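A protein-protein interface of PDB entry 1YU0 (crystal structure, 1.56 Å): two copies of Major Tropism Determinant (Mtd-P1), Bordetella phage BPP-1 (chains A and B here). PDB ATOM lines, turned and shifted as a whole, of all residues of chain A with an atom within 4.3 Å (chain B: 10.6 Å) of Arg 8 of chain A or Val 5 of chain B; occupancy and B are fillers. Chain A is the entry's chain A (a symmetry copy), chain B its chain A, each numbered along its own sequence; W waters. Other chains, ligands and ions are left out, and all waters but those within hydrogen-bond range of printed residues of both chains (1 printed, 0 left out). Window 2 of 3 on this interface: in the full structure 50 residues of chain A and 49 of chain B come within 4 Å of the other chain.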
ATOM      1  N   GLN A   6     -28.926 -18.515  -9.061  1.00  0.00           N
ATOM      2  CA  GLN A   6     -28.948 -19.146 -10.369  1.00  0.00           C
ATOM      3  C   GLN A   6     -29.898 -18.389 -11.275  1.00  0.00           C
ATOM      4  O   GLN A   6     -31.084 -18.213 -10.958  1.00  0.00           O
ATOM      5  CB  GLN A   6     -29.402 -20.599 -10.247  1.00  0.00           C
ATOM      6  CG  GLN A   6     -28.462 -21.454  -9.431  1.00  0.00           C
ATOM      7  CD  GLN A   6     -28.993 -22.857  -9.250  1.00  0.00           C
ATOM      8  OE1 GLN A   6     -28.788 -23.731 -10.094  1.00  0.00           O
ATOM      9  NE2 GLN A   6     -29.703 -23.079  -8.148  1.00  0.00           N
ATOM     10  N   PHE A   7     -29.389 -17.950 -12.416  1.00  0.00           N
ATOM     11  CA  PHE A   7     -30.182 -17.176 -13.339  1.00  0.00           C
ATOM     12  C   PHE A   7     -31.129 -18.048 -14.102  1.00  0.00           C
ATOM     13  O   PHE A   7     -30.903 -19.241 -14.251  1.00  0.00           O
ATOM     14  CB  PHE A   7     -29.285 -16.419 -14.314  1.00  0.00           C
ATOM     15  CG  PHE A   7     -28.552 -15.312 -13.661  1.00  0.00           C
ATOM     16  CD1 PHE A   7     -29.054 -14.029 -13.692  1.00  0.00           C
ATOM     17  CD2 PHE A   7     -27.416 -15.569 -12.924  1.00  0.00           C
ATOM     18  CE1 PHE A   7     -28.382 -13.011 -13.050  1.00  0.00           C
ATOM     19  CE2 PHE A   7     -26.755 -14.574 -12.278  1.00  0.00           C
ATOM     20  CZ  PHE A   7     -27.227 -13.289 -12.350  1.00  0.00           C
ATOM     21  N   ARG A   8     -32.198 -17.440 -14.583  1.00  0.00           N
ATOM     22  CA  ARG A   8     -33.109 -18.120 -15.473  1.00  0.00           C
ATOM     23  C   ARG A   8     -32.346 -18.527 -16.724  1.00  0.00           C
ATOM     24  O   ARG A   8     -31.417 -17.844 -17.173  1.00  0.00           O
ATOM     25  CB  ARG A   8     -34.307 -17.233 -15.796  1.00  0.00           C
ATOM     26  CG  ARG A   8     -35.229 -17.079 -14.581  1.00  0.00           C
ATOM     27  CD  ARG A   8     -35.863 -15.703 -14.463  1.00  0.00           C
ATOM     28  NE  ARG A   8     -36.383 -15.473 -13.112  1.00  0.00           N
ATOM     29  CZ  ARG A   8     -36.625 -14.278 -12.571  1.00  0.00           C
ATOM     30  NH1 ARG A   8     -36.399 -13.158 -13.252  1.00  0.00           N
ATOM     31  NH2 ARG A   8     -37.100 -14.199 -11.331  1.00  0.00           N
ATOM     32  N   GLY A   9     -32.712 -19.665 -17.270  1.00  0.00           N
ATOM     33  CA  GLY A   9     -31.962 -20.220 -18.359  1.00  0.00           C
ATOM     34  C   GLY A   9     -32.797 -21.043 -19.288  1.00  0.00           C
ATOM     35  O   GLY A   9     -33.973 -21.334 -19.027  1.00  0.00           O
ATOM     36  N   ARG A  23     -32.288  -5.250 -19.200  1.00  0.00           N
ATOM     37  CA  ARG A  23     -31.172  -5.439 -18.274  1.00  0.00           C
ATOM     38  C   ARG A  23     -31.286  -6.731 -17.469  1.00  0.00           C
ATOM     39  O   ARG A  23     -30.583  -6.898 -16.478  1.00  0.00           O
ATOM     40  CB  ARG A  23     -30.997  -4.232 -17.342  1.00  0.00           C
ATOM     41  CG  ARG A  23     -31.004  -2.898 -18.086  1.00  0.00           C
ATOM     42  CD  ARG A  23     -30.699  -1.725 -17.194  1.00  0.00           C
ATOM     43  NE  ARG A  23     -31.550  -1.670 -16.012  1.00  0.00           N
ATOM     44  CZ  ARG A  23     -32.810  -1.237 -15.994  1.00  0.00           C
ATOM     45  NH1 ARG A  23     -33.404  -0.786 -17.095  1.00  0.00           N
ATOM     46  NH2 ARG A  23     -33.487  -1.248 -14.856  1.00  0.00           N
ATOM     47  N   GLU A  24     -32.147  -7.643 -17.902  1.00  0.00           N
ATOM     48  CA  GLU A  24     -32.176  -8.997 -17.364  1.00  0.00           C
ATOM     49  C   GLU A  24     -31.063  -9.791 -18.030  1.00  0.00           C
ATOM     50  O   GLU A  24     -30.774  -9.576 -19.207  1.00  0.00           O
ATOM     51  CB  GLU A  24     -33.527  -9.656 -17.627  1.00  0.00           C
ATOM     52  CG  GLU A  24     -33.624 -11.070 -17.110  1.00  0.00           C
ATOM     53  CD  GLU A  24     -34.976 -11.713 -17.321  1.00  0.00           C
ATOM     54  OE1 GLU A  24     -35.875 -11.115 -17.972  1.00  0.00           O
ATOM     55  OE2 GLU A  24     -35.126 -12.848 -16.810  1.00  0.00           O
ATOM     56  N   THR A  26     -29.940 -13.824 -18.729  1.00  0.00           N
ATOM     57  CA  THR A  26     -30.260 -15.240 -18.681  1.00  0.00           C
ATOM     58  C   THR A  26     -29.027 -16.030 -19.102  1.00  0.00           C
ATOM     59  O   THR A  26     -28.034 -15.458 -19.544  1.00  0.00           O
ATOM     60  CB  THR A  26     -31.475 -15.592 -19.564  1.00  0.00           C
ATOM     61  OG1 THR A  26     -31.178 -15.314 -20.932  1.00  0.00           O
ATOM     62  CG2 THR A  26     -32.707 -14.794 -19.138  1.00  0.00           C
ATOM     63  N   VAL A  27     -29.080 -17.349 -18.911  1.00  0.00           N
ATOM     64  CA  VAL A  27     -27.999 -18.240 -19.330  1.00  0.00           C
ATOM     65  C   VAL A  27     -28.507 -19.189 -20.402  1.00  0.00           C
ATOM     66  O   VAL A  27     -29.514 -19.882 -20.213  1.00  0.00           O
ATOM     67  CB  VAL A  27     -27.434 -19.014 -18.128  1.00  0.00           C
ATOM     68  CG1 VAL A  27     -26.467 -20.095 -18.605  1.00  0.00           C
ATOM     69  CG2 VAL A  27     -26.738 -18.062 -17.156  1.00  0.00           C
ATOM     70  N   VAL B   5     -34.948 -10.458 -12.314  1.00  0.00           N
ATOM     71  CA  VAL B   5     -33.932  -9.508 -11.776  1.00  0.00           C
ATOM     72  C   VAL B   5     -33.318  -8.664 -12.894  1.00  0.00           C
ATOM     73  O   VAL B   5     -32.771  -9.197 -13.858  1.00  0.00           O
ATOM     74  CB  VAL B   5     -32.818 -10.245 -11.004  1.00  0.00           C
ATOM     75  CG1 VAL B   5     -31.717  -9.280 -10.573  1.00  0.00           C
ATOM     76  CG2 VAL B   5     -33.403 -10.952  -9.787  1.00  0.00           C
ATOM     77  N   GLN B   6     -33.420  -7.347 -12.745  1.00  0.00           N
ATOM     78  CA  GLN B   6     -32.879  -6.397 -13.702  1.00  0.00           C
ATOM     79  C   GLN B   6     -31.718  -5.656 -13.070  1.00  0.00           C
ATOM     80  O   GLN B   6     -31.857  -5.032 -12.007  1.00  0.00           O
ATOM     81  CB  GLN B   6     -33.957  -5.401 -14.123  1.00  0.00           C
ATOM     82  CG  GLN B   6     -35.118  -6.043 -14.845  1.00  0.00           C
ATOM     83  CD  GLN B   6     -36.207  -5.043 -15.159  1.00  0.00           C
ATOM     84  OE1 GLN B   6     -36.168  -4.357 -16.181  1.00  0.00           O
ATOM     85  NE2 GLN B   6     -37.184  -4.938 -14.263  1.00  0.00           N
ATOM     86  N   PHE B   7     -30.570  -5.704 -13.728  1.00  0.00           N
ATOM     87  CA  PHE B   7     -29.382  -5.078 -13.203  1.00  0.00           C
ATOM     88  C   PHE B   7     -29.424  -3.593 -13.395  1.00  0.00           C
ATOM     89  O   PHE B   7     -30.113  -3.092 -14.272  1.00  0.00           O
ATOM     90  CB  PHE B   7     -28.134  -5.645 -13.874  1.00  0.00           C
ATOM     91  CG  PHE B   7     -27.857  -7.039 -13.461  1.00  0.00           C
ATOM     92  CD1 PHE B   7     -26.980  -7.300 -12.431  1.00  0.00           C
ATOM     93  CD2 PHE B   7     -28.553  -8.084 -14.028  1.00  0.00           C
ATOM     94  CE1 PHE B   7     -26.755  -8.598 -12.029  1.00  0.00           C
ATOM     95  CE2 PHE B   7     -28.348  -9.365 -13.630  1.00  0.00           C
ATOM     96  CZ  PHE B   7     -27.438  -9.630 -12.639  1.00  0.00           C
ATOM     97  N   ARG B   8     -28.679  -2.893 -12.558  1.00  0.00           N
ATOM     98  CA  ARG B   8     -28.497  -1.471 -12.730  1.00  0.00           C
ATOM     99  C   ARG B   8     -27.832  -1.231 -14.077  1.00  0.00           C
ATOM    100  O   ARG B   8     -27.022  -2.033 -14.558  1.00  0.00           O
ATOM    101  CB  ARG B   8     -27.683  -0.891 -11.578  1.00  0.00           C
ATOM    102  CG  ARG B   8     -28.495  -0.873 -10.278  1.00  0.00           C
ATOM    103  CD  ARG B   8     -27.667  -1.155  -9.035  1.00  0.00           C
ATOM    104  NE  ARG B   8     -28.521  -1.531  -7.904  1.00  0.00           N
ATOM    105  CZ  ARG B   8     -28.119  -2.207  -6.826  1.00  0.00           C
ATOM    106  NH1 ARG B   8     -26.858  -2.608  -6.697  1.00  0.00           N
ATOM    107  NH2 ARG B   8     -28.992  -2.489  -5.862  1.00  0.00           N
ATOM    108  N   GLY B   9     -28.202  -0.138 -14.708  1.00  0.00           N
ATOM    109  CA  GLY B   9     -27.756   0.108 -16.048  1.00  0.00           C
ATOM    110  C   GLY B   9     -27.640   1.566 -16.369  1.00  0.00           C
ATOM    111  O   GLY B   9     -28.051   2.441 -15.594  1.00  0.00           O
ATOM    112  N   ILE B  25     -22.114  -6.283 -11.367  1.00  0.00           N
ATOM    113  CA  ILE B  25     -22.376  -6.277 -12.807  1.00  0.00           C
ATOM    114  C   ILE B  25     -23.400  -5.185 -13.101  1.00  0.00           C
ATOM    115  O   ILE B  25     -24.393  -5.061 -12.376  1.00  0.00           O
ATOM    116  CB  ILE B  25     -22.957  -7.640 -13.255  1.00  0.00           C
ATOM    117  CG1 ILE B  25     -21.825  -8.651 -13.405  1.00  0.00           C
ATOM    118  CG2 ILE B  25     -23.788  -7.510 -14.530  1.00  0.00           C
ATOM    119  CD1 ILE B  25     -22.310 -10.076 -13.592  1.00  0.00           C
ATOM    120  N   THR B  26     -23.136  -4.374 -14.126  1.00  0.00           N
ATOM    121  CA  THR B  26     -24.132  -3.458 -14.656  1.00  0.00           C
ATOM    122  C   THR B  26     -24.329  -3.760 -16.136  1.00  0.00           C
ATOM    123  O   THR B  26     -23.599  -4.558 -16.718  1.00  0.00           O
ATOM    124  CB  THR B  26     -23.740  -1.982 -14.436  1.00  0.00           C
ATOM    125  OG1 THR B  26     -22.536  -1.690 -15.145  1.00  0.00           O
ATOM    126  CG2 THR B  26     -23.540  -1.687 -12.950  1.00  0.00           C
ATOM    127  N   VAL B  27     -25.360  -3.154 -16.728  1.00  0.00           N
ATOM    128  CA  VAL B  27     -25.630  -3.297 -18.158  1.00  0.00           C
ATOM    129  C   VAL B  27     -25.487  -1.947 -18.841  1.00  0.00           C
ATOM    130  O   VAL B  27     -26.112  -0.960 -18.436  1.00  0.00           O
ATOM    131  CB  VAL B  27     -27.029  -3.890 -18.392  1.00  0.00           C
ATOM    132  CG1 VAL B  27     -27.386  -3.828 -19.874  1.00  0.00           C
ATOM    133  CG2 VAL B  27     -27.092  -5.330 -17.884  1.00  0.00           C
ATOM    134  N   VAL B  34     -22.842  -6.596 -20.786  1.00  0.00           N
ATOM    135  CA  VAL B  34     -22.526  -6.594 -19.360  1.00  0.00           C
ATOM    136  C   VAL B  34     -21.225  -5.833 -19.136  1.00  0.00           C
ATOM    137  O   VAL B  34     -20.307  -5.907 -19.943  1.00  0.00           O
ATOM    138  CB  VAL B  34     -22.374  -8.046 -18.847  1.00  0.00           C
ATOM    139  CG1 VAL B  34     -21.526  -8.137 -17.573  1.00  0.00           C
ATOM    140  CG2 VAL B  34     -23.754  -8.645 -18.664  1.00  0.00           C
HETATM  141  O   HOH W   1     -32.630  -2.359 -11.925  1.00  0.00           O
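The guanidinium group (NE) of Arg 23 of chain A lies within hydrogen-bond range of the backbone carbonyl oxygen (O) of Phe 7 of chain B.
The guanidinium group (NH1) of Arg 8 of chain A sits close to the backbone NH (N) of Val 5 of chain B.
The side-chain carboxylate (OE2) of Glu 24 of chain A lies within salt-bridge range of the guanidinium group (NH1) of Arg 8 of chain A, at 3.8 Å.
The backbone carbonyl oxygen (O) of Arg 8 of chain A is in hydrogen-bond range of the backbone NH (N) of Val 27 of chain A (3.0 Å).
Among the printed residues, merely in contact across the chains: Phe 7 of chain A with Phe 7 of chain B (3.5 Å), Glu 24 of chain A with Val 5 of chain B (3.6 Å), Arg 23 of chain A with Gln 6 of chain B (3.6 Å) and Arg 23 of chain A with Gly 9 of chain B (3.7 Å).
Gln 6 of chain A touches none of the printed residues of chain B.
Of the printed residues of chain B, Phe 7 of chain A touches Phe 7 (3.5 Å).
Of chain B, only Val 5 comes within 4 Å of Arg 8 of chain A.
No residue of chain B comes within 4 Å of Gly 9 of chain A.
Glu 24 of chain A touches one residue of chain B.
No residue of chain B comes within 4 Å of Val 27 of chain A.
Val 5 of chain B touches just these residues of chain A: Arg 8 and Glu 24.
Of the printed residues of chain A, Gln 6 of chain B touches Arg 23.
Of the printed residues of chain A, Phe 7 of chain B touches Phe 7 and Arg 23.
Printed residues of chain A within 4 Å of Gly 9 of chain B: Arg 23 (3.7 Å).
The nearest residue of chain B that does not touch Arg 8 of chain A is Gln 6 of chain B (6.5 Å).
Printed residues of chain B that touch a printed residue of chain A: Val 5, Gln 6, Phe 7 and Gly 9.
Hydrophobic or aromatic side chains of chain B within 4 Å of the printed part of chain A: Phe 7.
Of the 8 printed residues of chain A, 4 touch a printed residue of chain B.
Phe 7 of chain B touches its own counterpart, Phe 7 of chain A.
6 positions are printed for both chains.
Of the 6 pairs that touch across the chains among the printed residues, 1 has its exchanged pair printed and touching as well.
Water W1 bridges the backbone carbonyl oxygen (O) of Gln 6 of chain B and the guanidinium group (NH2) of Arg 23 of chain A.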
